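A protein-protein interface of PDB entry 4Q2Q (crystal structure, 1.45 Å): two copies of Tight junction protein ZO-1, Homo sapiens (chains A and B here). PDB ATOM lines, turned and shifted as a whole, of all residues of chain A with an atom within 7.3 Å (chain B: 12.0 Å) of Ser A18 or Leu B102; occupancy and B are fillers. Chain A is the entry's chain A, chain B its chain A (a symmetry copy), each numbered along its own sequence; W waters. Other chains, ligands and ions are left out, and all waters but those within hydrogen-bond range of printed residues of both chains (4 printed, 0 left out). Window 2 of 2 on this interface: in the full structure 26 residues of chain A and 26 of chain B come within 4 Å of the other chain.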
ATOM      1  N   PHE A  13      -7.486 -25.687  21.778  1.00  0.00           N
ATOM      2  CA  PHE A  13      -6.122 -26.232  21.921  1.00  0.00           C
ATOM      3  C   PHE A  13      -5.141 -25.278  21.259  1.00  0.00           C
ATOM      4  O   PHE A  13      -5.522 -24.485  20.388  1.00  0.00           O
ATOM      5  CB  PHE A  13      -6.008 -27.625  21.281  1.00  0.00           C
ATOM      6  CG  PHE A  13      -6.397 -27.683  19.831  1.00  0.00           C
ATOM      7  CD1 PHE A  13      -7.715 -27.867  19.456  1.00  0.00           C
ATOM      8  CD2 PHE A  13      -5.439 -27.626  18.830  1.00  0.00           C
ATOM      9  CE1 PHE A  13      -8.068 -27.924  18.141  1.00  0.00           C
ATOM     10  CE2 PHE A  13      -5.804 -27.688  17.492  1.00  0.00           C
ATOM     11  CZ  PHE A  13      -7.118 -27.852  17.155  1.00  0.00           C
ATOM     12  N   ARG A  14      -3.872 -25.393  21.647  1.00  0.00           N
ATOM     13  CA  ARG A  14      -2.806 -24.665  20.978  1.00  0.00           C
ATOM     14  C   ARG A  14      -2.381 -25.408  19.713  1.00  0.00           C
ATOM     15  O   ARG A  14      -2.006 -26.582  19.772  1.00  0.00           O
ATOM     16  CB  ARG A  14      -1.606 -24.521  21.916  1.00  0.00           C
ATOM     17  CG  ARG A  14      -0.402 -23.863  21.280  1.00  0.00           C
ATOM     18  CD  ARG A  14       0.893 -24.079  22.092  1.00  0.00           C
ATOM     19  NE  ARG A  14       1.551 -25.370  21.817  1.00  0.00           N
ATOM     20  CZ  ARG A  14       2.306 -25.655  20.750  1.00  0.00           C
ATOM     21  NH1 ARG A  14       2.518 -24.763  19.790  1.00  0.00           N
ATOM     22  NH2 ARG A  14       2.852 -26.866  20.630  1.00  0.00           N
ATOM     23  N   LYS A  15      -2.409 -24.728  18.568  1.00  0.00           N
ATOM     24  CA  LYS A  15      -1.980 -25.351  17.324  1.00  0.00           C
ATOM     25  C   LYS A  15      -0.481 -25.654  17.400  1.00  0.00           C
ATOM     26  O   LYS A  15       0.318 -24.784  17.768  1.00  0.00           O
ATOM     27  CB  LYS A  15      -2.256 -24.439  16.128  1.00  0.00           C
ATOM     28  CG  LYS A  15      -1.988 -25.127  14.832  1.00  0.00           C
ATOM     29  CD  LYS A  15      -2.124 -24.250  13.617  1.00  0.00           C
ATOM     30  CE  LYS A  15      -1.535 -24.922  12.397  1.00  0.00           C
ATOM     31  NZ  LYS A  15      -1.856 -24.293  11.103  1.00  0.00           N
ATOM     32  N   GLY A  16      -0.127 -26.896  17.059  1.00  0.00           N
ATOM     33  CA  GLY A  16       1.247 -27.293  16.839  1.00  0.00           C
ATOM     34  C   GLY A  16       1.624 -27.047  15.397  1.00  0.00           C
ATOM     35  O   GLY A  16       1.234 -26.043  14.803  1.00  0.00           O
ATOM     36  N   ASP A  17       2.393 -27.971  14.816  1.00  0.00           N
ATOM     37  CA  ASP A  17       2.808 -27.836  13.434  1.00  0.00           C
ATOM     38  C   ASP A  17       1.652 -27.975  12.422  1.00  0.00           C
ATOM     39  O   ASP A  17       1.716 -27.452  11.304  1.00  0.00           O
ATOM     40  CB  ASP A  17       3.908 -28.847  13.130  1.00  0.00           C
ATOM     41  CG  ASP A  17       5.170 -28.599  13.938  1.00  0.00           C
ATOM     42  OD1 ASP A  17       5.844 -27.590  13.702  1.00  0.00           O
ATOM     43  OD2 ASP A  17       5.460 -29.384  14.842  1.00  0.00           O
ATOM     44  N   SER A  18       0.611 -28.701  12.799  1.00  0.00           N
ATOM     45  CA  SER A  18      -0.619 -28.813  11.982  1.00  0.00           C
ATOM     46  C   SER A  18      -1.787 -28.776  12.949  1.00  0.00           C
ATOM     47  O   SER A  18      -1.585 -28.932  14.165  1.00  0.00           O
ATOM     48  CB  SER A  18      -0.631 -30.117  11.187  1.00  0.00           C
ATOM     49  OG  SER A  18       0.455 -30.180  10.278  1.00  0.00           O
ATOM     50  N   VAL A  19      -3.012 -28.572  12.442  1.00  0.00           N
ATOM     51  CA  VAL A  19      -4.171 -28.492  13.351  1.00  0.00           C
ATOM     52  C   VAL A  19      -4.642 -29.870  13.806  1.00  0.00           C
ATOM     53  O   VAL A  19      -5.348 -29.962  14.831  1.00  0.00           O
ATOM     54  CB  VAL A  19      -5.418 -27.717  12.805  1.00  0.00           C
ATOM     55  CG1 VAL A  19      -5.163 -26.231  12.769  1.00  0.00           C
ATOM     56  CG2 VAL A  19      -5.835 -28.234  11.446  1.00  0.00           C
ATOM     57  N   GLY A  20      -4.250 -30.938  13.095  1.00  0.00           N
ATOM     58  CA  GLY A  20      -4.601 -32.309  13.530  1.00  0.00           C
ATOM     59  C   GLY A  20      -5.977 -32.808  13.168  1.00  0.00           C
ATOM     60  O   GLY A  20      -6.536 -33.658  13.883  1.00  0.00           O
ATOM     61  N   LEU A  21      -6.497 -32.303  12.058  1.00  0.00           N
ATOM     62  CA  LEU A  21      -7.864 -32.551  11.583  1.00  0.00           C
ATOM     63  C   LEU A  21      -7.858 -32.784  10.074  1.00  0.00           C
ATOM     64  O   LEU A  21      -7.017 -32.209   9.374  1.00  0.00           O
ATOM     65  CB  LEU A  21      -8.754 -31.314  11.828  1.00  0.00           C
ATOM     66  CG  LEU A  21      -9.113 -30.892  13.254  1.00  0.00           C
ATOM     67  CD1 LEU A  21     -10.011 -29.647  13.270  1.00  0.00           C
ATOM     68  CD2 LEU A  21      -9.778 -32.040  13.982  1.00  0.00           C
ATOM     69  N   ARG A  22      -8.838 -33.550   9.576  1.00  0.00           N
ATOM     70  CA  ARG A  22      -9.186 -33.549   8.174  1.00  0.00           C
ATOM     71  C   ARG A  22     -10.663 -33.218   8.082  1.00  0.00           C
ATOM     72  O   ARG A  22     -11.427 -33.470   9.028  1.00  0.00           O
ATOM     73  CB  ARG A  22      -8.792 -34.849   7.458  1.00  0.00           C
ATOM     74  CG  ARG A  22      -9.315 -36.108   8.023  1.00  0.00           C
ATOM     75  CD  ARG A  22      -8.588 -37.323   7.397  1.00  0.00           C
ATOM     76  NE  ARG A  22      -8.483 -37.190   5.960  1.00  0.00           N
ATOM     77  CZ  ARG A  22      -7.856 -38.052   5.156  1.00  0.00           C
ATOM     78  NH1 ARG A  22      -7.222 -39.136   5.655  1.00  0.00           N
ATOM     79  NH2 ARG A  22      -7.812 -37.788   3.852  1.00  0.00           N
ATOM     80  N   LEU A  23     -11.068 -32.660   6.936  1.00  0.00           N
ATOM     81  CA  LEU A  23     -12.421 -32.133   6.710  1.00  0.00           C
ATOM     82  C   LEU A  23     -13.143 -32.912   5.608  1.00  0.00           C
ATOM     83  O   LEU A  23     -12.525 -33.487   4.704  1.00  0.00           O
ATOM     84  CB  LEU A  23     -12.360 -30.659   6.276  1.00  0.00           C
ATOM     85  CG  LEU A  23     -11.724 -29.657   7.221  1.00  0.00           C
ATOM     86  CD1 LEU A  23     -11.737 -28.272   6.623  1.00  0.00           C
ATOM     87  CD2 LEU A  23     -12.358 -29.694   8.585  1.00  0.00           C
ATOM     88  N   LEU A  37      -6.336 -36.517  14.375  1.00  0.00           N
ATOM     89  CA  LEU A  37      -5.037 -37.160  14.414  1.00  0.00           C
ATOM     90  C   LEU A  37      -4.810 -37.774  15.787  1.00  0.00           C
ATOM     91  O   LEU A  37      -5.054 -37.143  16.821  1.00  0.00           O
ATOM     92  CB  LEU A  37      -3.978 -36.101  14.120  1.00  0.00           C
ATOM     93  CG  LEU A  37      -2.756 -36.525  13.361  1.00  0.00           C
ATOM     94  CD1 LEU A  37      -2.972 -37.307  11.995  1.00  0.00           C
ATOM     95  CD2 LEU A  37      -1.802 -35.299  13.165  1.00  0.00           C
ATOM     96  N   SER A  40      -2.901 -36.120  19.062  1.00  0.00           N
ATOM     97  CA  SER A  40      -2.846 -34.674  18.830  1.00  0.00           C
ATOM     98  C   SER A  40      -3.568 -33.901  19.931  1.00  0.00           C
ATOM     99  O   SER A  40      -4.422 -34.448  20.633  1.00  0.00           O
ATOM    100  CB  SER A  40      -3.517 -34.301  17.509  1.00  0.00           C
ATOM    101  OG  SER A  40      -4.934 -34.564  17.533  1.00  0.00           O
ATOM    102  N   PRO A  41      -3.254 -32.605  20.067  1.00  0.00           N
ATOM    103  CA  PRO A  41      -4.026 -31.729  20.949  1.00  0.00           C
ATOM    104  C   PRO A  41      -5.525 -31.777  20.644  1.00  0.00           C
ATOM    105  O   PRO A  41      -6.342 -31.800  21.565  1.00  0.00           O
ATOM    106  CB  PRO A  41      -3.452 -30.341  20.635  1.00  0.00           C
ATOM    107  CG  PRO A  41      -2.010 -30.618  20.222  1.00  0.00           C
ATOM    108  CD  PRO A  41      -2.088 -31.920  19.465  1.00  0.00           C
ATOM    109  N   ALA A  69     -12.033 -22.850   3.966  1.00  0.00           N
ATOM    110  CA  ALA A  69     -12.080 -23.646   5.234  1.00  0.00           C
ATOM    111  C   ALA A  69     -10.740 -24.389   5.418  1.00  0.00           C
ATOM    112  O   ALA A  69     -10.131 -24.369   6.474  1.00  0.00           O
ATOM    113  CB  ALA A  69     -13.241 -24.649   5.209  1.00  0.00           C
ATOM    114  N   VAL A  70     -10.260 -24.965   4.331  1.00  0.00           N
ATOM    115  CA  VAL A  70      -8.992 -25.660   4.341  1.00  0.00           C
ATOM    116  C   VAL A  70      -7.816 -24.715   4.574  1.00  0.00           C
ATOM    117  O   VAL A  70      -7.009 -24.969   5.460  1.00  0.00           O
ATOM    118  CB  VAL A  70      -8.799 -26.454   3.014  1.00  0.00           C
ATOM    119  CG1 VAL A  70      -7.361 -26.991   2.897  1.00  0.00           C
ATOM    120  CG2 VAL A  70      -9.813 -27.589   2.929  1.00  0.00           C
ATOM    121  N   LEU A  71      -7.707 -23.659   3.759  1.00  0.00           N
ATOM    122  CA  LEU A  71      -6.567 -22.765   3.846  1.00  0.00           C
ATOM    123  C   LEU A  71      -6.527 -21.987   5.154  1.00  0.00           C
ATOM    124  O   LEU A  71      -5.451 -21.742   5.701  1.00  0.00           O
ATOM    125  CB  LEU A  71      -6.506 -21.824   2.644  1.00  0.00           C
ATOM    126  CG  LEU A  71      -5.868 -22.373   1.360  1.00  0.00           C
ATOM    127  CD1 LEU A  71      -6.167 -21.453   0.209  1.00  0.00           C
ATOM    128  CD2 LEU A  71      -4.389 -22.494   1.516  1.00  0.00           C
ATOM    129  N   PHE A  72      -7.697 -21.586   5.659  1.00  0.00           N
ATOM    130  CA  PHE A  72      -7.751 -20.905   6.935  1.00  0.00           C
ATOM    131  C   PHE A  72      -7.066 -21.743   8.017  1.00  0.00           C
ATOM    132  O   PHE A  72      -6.256 -21.249   8.798  1.00  0.00           O
ATOM    133  CB  PHE A  72      -9.211 -20.603   7.307  1.00  0.00           C
ATOM    134  CG  PHE A  72      -9.349 -19.968   8.642  1.00  0.00           C
ATOM    135  CD1 PHE A  72      -9.087 -18.646   8.814  1.00  0.00           C
ATOM    136  CD2 PHE A  72      -9.778 -20.689   9.714  1.00  0.00           C
ATOM    137  CE1 PHE A  72      -9.204 -18.081  10.057  1.00  0.00           C
ATOM    138  CE2 PHE A  72      -9.865 -20.105  10.963  1.00  0.00           C
ATOM    139  CZ  PHE A  72      -9.586 -18.808  11.117  1.00  0.00           C
ATOM    140  N   LEU A  73      -7.407 -23.018   8.094  1.00  0.00           N
ATOM    141  CA  LEU A  73      -6.858 -23.879   9.155  1.00  0.00           C
ATOM    142  C   LEU A  73      -5.369 -24.143   8.921  1.00  0.00           C
ATOM    143  O   LEU A  73      -4.566 -24.068   9.853  1.00  0.00           O
ATOM    144  CB  LEU A  73      -7.634 -25.192   9.200  1.00  0.00           C
ATOM    145  CG  LEU A  73      -9.058 -25.065   9.733  1.00  0.00           C
ATOM    146  CD1 LEU A  73      -9.800 -26.367   9.598  1.00  0.00           C
ATOM    147  CD2 LEU A  73      -9.126 -24.563  11.146  1.00  0.00           C
ATOM    148  N   LEU A  74      -4.987 -24.373   7.683  1.00  0.00           N
ATOM    149  CA  LEU A  74      -3.545 -24.539   7.371  1.00  0.00           C
ATOM    150  C   LEU A  74      -2.689 -23.341   7.756  1.00  0.00           C
ATOM    151  O   LEU A  74      -1.534 -23.492   8.202  1.00  0.00           O
ATOM    152  CB  LEU A  74      -3.363 -24.788   5.879  1.00  0.00           C
ATOM    153  CG  LEU A  74      -3.670 -26.162   5.355  1.00  0.00           C
ATOM    154  CD1 LEU A  74      -3.402 -26.121   3.861  1.00  0.00           C
ATOM    155  CD2 LEU A  74      -2.749 -27.193   6.041  1.00  0.00           C
ATOM    156  N   ASP A  75      -3.225 -22.159   7.524  1.00  0.00           N
ATOM    157  CA  ASP A  75      -2.448 -20.931   7.708  1.00  0.00           C
ATOM    158  C   ASP A  75      -2.394 -20.388   9.131  1.00  0.00           C
ATOM    159  O   ASP A  75      -1.551 -19.539   9.411  1.00  0.00           O
ATOM    160  CB  ASP A  75      -2.958 -19.869   6.776  1.00  0.00           C
ATOM    161  CG  ASP A  75      -1.912 -18.875   6.405  1.00  0.00           C
ATOM    162  OD1 ASP A  75      -0.692 -19.199   6.378  1.00  0.00           O
ATOM    163  OD2 ASP A  75      -2.343 -17.745   6.180  1.00  0.00           O
ATOM    164  N   LEU A  76      -3.235 -20.874  10.048  1.00  0.00           N
ATOM    165  CA  LEU A  76      -3.132 -20.405  11.428  1.00  0.00           C
ATOM    166  C   LEU A  76      -1.709 -20.661  11.922  1.00  0.00           C
ATOM    167  O   LEU A  76      -1.156 -21.736  11.670  1.00  0.00           O
ATOM    168  CB  LEU A  76      -4.120 -21.111  12.346  1.00  0.00           C
ATOM    169  CG  LEU A  76      -5.562 -20.720  12.213  1.00  0.00           C
ATOM    170  CD1 LEU A  76      -6.433 -21.712  13.006  1.00  0.00           C
ATOM    171  CD2 LEU A  76      -5.705 -19.251  12.657  1.00  0.00           C
ATOM    172  N   LYS A  78       1.506 -21.636  14.172  1.00  0.00           N
ATOM    173  CA  LYS A  78       1.898 -22.471  15.281  1.00  0.00           C
ATOM    174  C   LYS A  78       1.902 -21.685  16.572  1.00  0.00           C
ATOM    175  O   LYS A  78       2.441 -20.574  16.633  1.00  0.00           O
ATOM    176  CB  LYS A  78       3.309 -23.065  15.032  1.00  0.00           C
ATOM    177  CG  LYS A  78       3.764 -24.021  16.105  1.00  0.00           C
ATOM    178  CD  LYS A  78       5.098 -24.622  15.746  1.00  0.00           C
ATOM    179  CE  LYS A  78       5.472 -25.639  16.757  1.00  0.00           C
ATOM    180  NZ  LYS A  78       6.809 -26.182  16.405  1.00  0.00           N
ATOM    181  N   VAL A  82      -6.530 -22.356  19.017  1.00  0.00           N
ATOM    182  CA  VAL A  82      -7.625 -22.647  18.108  1.00  0.00           C
ATOM    183  C   VAL A  82      -8.846 -22.994  18.957  1.00  0.00           C
ATOM    184  O   VAL A  82      -8.793 -23.864  19.823  1.00  0.00           O
ATOM    185  CB  VAL A  82      -7.278 -23.882  17.205  1.00  0.00           C
ATOM    186  CG1 VAL A  82      -8.412 -24.190  16.223  1.00  0.00           C
ATOM    187  CG2 VAL A  82      -5.970 -23.687  16.476  1.00  0.00           C
ATOM    188  N   GLU B  49      -9.350 -43.222   2.798  1.00  0.00           N
ATOM    189  CA  GLU B  49     -10.390 -42.247   3.129  1.00  0.00           C
ATOM    190  C   GLU B  49     -10.585 -41.359   1.903  1.00  0.00           C
ATOM    191  O   GLU B  49      -9.611 -40.951   1.255  1.00  0.00           O
ATOM    192  CB  GLU B  49     -10.009 -41.438   4.377  1.00  0.00           C
ATOM    193  CG  GLU B  49     -11.035 -40.384   4.742  1.00  0.00           C
ATOM    194  CD  GLU B  49     -11.116 -39.967   6.185  1.00  0.00           C
ATOM    195  OE1 GLU B  49     -10.361 -40.485   7.035  1.00  0.00           O
ATOM    196  OE2 GLU B  49     -11.990 -39.084   6.461  1.00  0.00           O
ATOM    197  N   TRP B  97     -16.657 -34.327  -0.753  1.00  0.00           N
ATOM    198  CA  TRP B  97     -15.235 -34.061  -0.828  1.00  0.00           C
ATOM    199  C   TRP B  97     -14.578 -34.311   0.534  1.00  0.00           C
ATOM    200  O   TRP B  97     -15.212 -34.180   1.567  1.00  0.00           O
ATOM    201  CB  TRP B  97     -14.922 -32.625  -1.312  1.00  0.00           C
ATOM    202  CG  TRP B  97     -15.548 -31.564  -0.476  1.00  0.00           C
ATOM    203  CD1 TRP B  97     -16.748 -30.989  -0.693  1.00  0.00           C
ATOM    204  CD2 TRP B  97     -15.022 -30.951   0.730  1.00  0.00           C
ATOM    205  NE1 TRP B  97     -17.019 -30.079   0.290  1.00  0.00           N
ATOM    206  CE2 TRP B  97     -15.981 -30.032   1.172  1.00  0.00           C
ATOM    207  CE3 TRP B  97     -13.847 -31.089   1.454  1.00  0.00           C
ATOM    208  CZ2 TRP B  97     -15.806 -29.252   2.321  1.00  0.00           C
ATOM    209  CZ3 TRP B  97     -13.668 -30.330   2.604  1.00  0.00           C
ATOM    210  CH2 TRP B  97     -14.633 -29.414   3.019  1.00  0.00           C
ATOM    211  N   PHE B  98     -13.282 -34.640   0.496  1.00  0.00           N
ATOM    212  CA  PHE B  98     -12.476 -34.890   1.675  1.00  0.00           C
ATOM    213  C   PHE B  98     -11.125 -34.189   1.517  1.00  0.00           C
ATOM    214  O   PHE B  98     -10.442 -34.353   0.491  1.00  0.00           O
ATOM    215  CB  PHE B  98     -12.198 -36.405   1.822  1.00  0.00           C
ATOM    216  CG  PHE B  98     -13.416 -37.216   2.224  1.00  0.00           C
ATOM    217  CD1 PHE B  98     -14.390 -37.534   1.307  1.00  0.00           C
ATOM    218  CD2 PHE B  98     -13.555 -37.682   3.530  1.00  0.00           C
ATOM    219  CE1 PHE B  98     -15.500 -38.265   1.691  1.00  0.00           C
ATOM    220  CE2 PHE B  98     -14.668 -38.427   3.919  1.00  0.00           C
ATOM    221  CZ  PHE B  98     -15.612 -38.727   2.992  1.00  0.00           C
ATOM    222  N   SER B  99     -10.727 -33.437   2.528  1.00  0.00           N
ATOM    223  CA  SER B  99      -9.418 -32.794   2.526  1.00  0.00           C
ATOM    224  C   SER B  99      -8.354 -33.786   2.923  1.00  0.00           C
ATOM    225  O   SER B  99      -8.650 -34.859   3.422  1.00  0.00           O
ATOM    226  CB  SER B  99      -9.377 -31.599   3.488  1.00  0.00           C
ATOM    227  OG  SER B  99      -9.230 -32.019   4.828  1.00  0.00           O
ATOM    228  N   ASP B 100      -7.107 -33.394   2.722  1.00  0.00           N
ATOM    229  CA  ASP B 100      -5.989 -34.069   3.336  1.00  0.00           C
ATOM    230  C   ASP B 100      -5.907 -33.664   4.815  1.00  0.00           C
ATOM    231  O   ASP B 100      -6.639 -32.811   5.293  1.00  0.00           O
ATOM    232  CB  ASP B 100      -4.701 -33.673   2.611  1.00  0.00           C
ATOM    233  CG  ASP B 100      -4.720 -34.019   1.126  1.00  0.00           C
ATOM    234  OD1 ASP B 100      -5.301 -35.056   0.733  1.00  0.00           O
ATOM    235  OD2 ASP B 100      -4.137 -33.247   0.336  1.00  0.00           O
ATOM    236  N   TRP B 101      -5.021 -34.298   5.571  1.00  0.00           N
ATOM    237  CA  TRP B 101      -4.695 -33.863   6.914  1.00  0.00           C
ATOM    238  C   TRP B 101      -4.190 -32.418   6.881  1.00  0.00           C
ATOM    239  O   TRP B 101      -3.346 -32.066   6.049  1.00  0.00           O
ATOM    240  CB  TRP B 101      -3.618 -34.753   7.514  1.00  0.00           C
ATOM    241  CG  TRP B 101      -4.121 -36.124   7.952  1.00  0.00           C
ATOM    242  CD1 TRP B 101      -3.833 -37.320   7.383  1.00  0.00           C
ATOM    243  CD2 TRP B 101      -5.028 -36.401   9.017  1.00  0.00           C
ATOM    244  NE1 TRP B 101      -4.455 -38.340   8.056  1.00  0.00           N
ATOM    245  CE2 TRP B 101      -5.207 -37.804   9.061  1.00  0.00           C
ATOM    246  CE3 TRP B 101      -5.709 -35.611   9.938  1.00  0.00           C
ATOM    247  CZ2 TRP B 101      -6.046 -38.419   9.984  1.00  0.00           C
ATOM    248  CZ3 TRP B 101      -6.536 -36.227  10.862  1.00  0.00           C
ATOM    249  CH2 TRP B 101      -6.696 -37.626  10.878  1.00  0.00           C
ATOM    250  N   LEU B 102      -4.722 -31.606   7.802  1.00  0.00           N
ATOM    251  CA  LEU B 102      -4.412 -30.194   7.944  1.00  0.00           C
ATOM    252  C   LEU B 102      -3.841 -29.967   9.324  1.00  0.00           C
ATOM    253  O   LEU B 102      -3.221 -28.902   9.544  1.00  0.00           O
ATOM    254  CB  LEU B 102      -5.686 -29.358   7.816  1.00  0.00           C
ATOM    255  CG  LEU B 102      -6.630 -29.641   6.637  1.00  0.00           C
ATOM    256  CD1 LEU B 102      -7.868 -28.756   6.762  1.00  0.00           C
ATOM    257  CD2 LEU B 102      -5.914 -29.531   5.291  1.00  0.00           C
ATOM    258  OXT LEU B 102      -4.039 -30.761  10.271  1.00  0.00           O
HETATM  259  O   HOH W   1      -0.349 -28.846   8.201  1.00  0.00           O
HETATM  260  O   HOH W   2     -10.813 -35.821   4.689  1.00  0.00           O
HETATM  261  O   HOH W   3      -7.359 -40.747   7.798  1.00  0.00           O
HETATM  262  O   HOH W   4      -7.162 -40.097   1.892  1.00  0.00           O
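The backbone carbonyl oxygen of Leu A23 sits at hydrogen-bond distance from the backbone NH of Ser B99, 2.8 Å away. The backbone carbonyl oxygen (O) of Ser B99 is in hydrogen-bond range of the guanidinium group (NH2) of Arg A22, at 3.1 Å. OE1 of Glu B49 is in salt-bridge range of NH1 of Arg A22 (3.7 Å). The backbone carbonyl oxygen of Leu A21 lies within hydrogen-bond range of the backbone NH of Leu B102 (2.8 Å). The backbone NH of Gly A20 lies within hydrogen-bond range of the chain-end carboxylate of Leu B102. N of Val A19 is in hydrogen-bond range of O of Leu B102, at 2.9 Å.
Water W1 lies within hydrogen-bond range of the side-chain hydroxyl of Ser A18 (2.6 Å) and the chain-end carboxylate of Leu B102 (3.2 Å). Water W4 bridges O of Glu B49 (2.7 Å) and NH2 of Arg A22 (3.1 Å). Water W2 lies within hydrogen-bond range of the backbone carbonyl oxygen (O) of Ser B99, the backbone carbonyl oxygen (O) of Leu A23 and the guanidinium group (NE) of Arg A22. Water W3 lies within hydrogen-bond range of the guanidinium group (NH1) of Arg A22 (2.7 Å) and the side-chain carboxylate (OE1) of Glu B49 (3.1 Å).
The side-chain amino group (NZ) of Lys A15 lies within hydrogen-bond range of the backbone carbonyl oxygen (O) of Leu A74 (3.0 Å). O of Gly A20 sits at hydrogen-bond distance from N of Leu A37, at 2.9 Å. O of Leu A37 sits at hydrogen-bond distance from OG of Ser A40 (2.7 Å).
Of the printed residues of chain A, Leu B102 touches Ser A18 (3.3 Å), Val A19 (2.9 Å), Gly A20 (2.8 Å), Leu A21 (2.8 Å), Leu A23 (3.9 Å), Val A70 (3.8 Å) and Leu A74 (3.9 Å). No residue of chain B comes within 4 Å of Gly A16. Leu A23 touches just these residues of chain B: Trp B97 (3.9 Å), Phe B98 (3.3 Å), Ser B99 (2.8 Å) and Leu B102 (3.9 Å). No residue of chain B comes within 4 Å of Ala A69. Of chain B, only Leu B102 (3.8 Å) comes within 4 Å of Val A70. Leu A73 touches none of the printed residues of chain B. Of the printed residues of chain B, Val A19 touches Leu B102 (2.9 Å). Printed residues of chain B within 4 Å of Leu A37: Trp B101 (3.5 Å). Of the printed residues of chain A, Trp B101 touches Gly A20 (3.97 Å), Leu A21 (3.6 Å), Arg A22 (3.7 Å) and Leu A37 (3.5 Å). Of the printed residues of chain A, Asp B100 touches Arg A22. The nearest printed residue of chain B that does not touch Ser A18 is Trp B101 (6.0 Å). The nearest printed residue of chain A that does not touch Leu B102 is Leu A73 (4.2 Å).
No position is printed for both chains. Of the 17 pairs that touch across the chains among the printed residues, none has its exchanged pair printed and touching as well.
Hydrophobic or aromatic side chains of chain B within 4 Å of the printed part of chain A: Trp B97, Trp B101 and Leu B102. Printed residues of chain A that touch a printed residue of chain B: Ser A18, Val A19, Gly A20, Leu A21, Arg A22, Leu A23, Leu A37, Val A70 and Leu A74. Among the printed residues, 17 pairs touch across the chains. Among the printed residues, Asp or Glu carboxylates within 4 Å of a Lys or Arg side-chain nitrogen of the other chain: Arg A22 with Glu B49 (3.7 Å).
Among the printed residues, pairs that only touch across the chains: Ser A18 with Leu B102 (3.3 Å), Leu A23 with Phe B98 (3.3 Å), Leu A37 with Trp B101 (3.5 Å), Leu A21 with Trp B101 (3.6 Å), Arg A22 with Asp B100 (3.7 Å), Arg A22 with Trp B101 (3.7 Å), Val A70 with Leu B102 (3.8 Å), Leu A23 with Leu B102 (3.9 Å), Leu A23 with Trp B97 (3.9 Å), Leu A74 with Leu B102 (3.9 Å) and Gly A20 with Trp B101 (3.97 Å).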
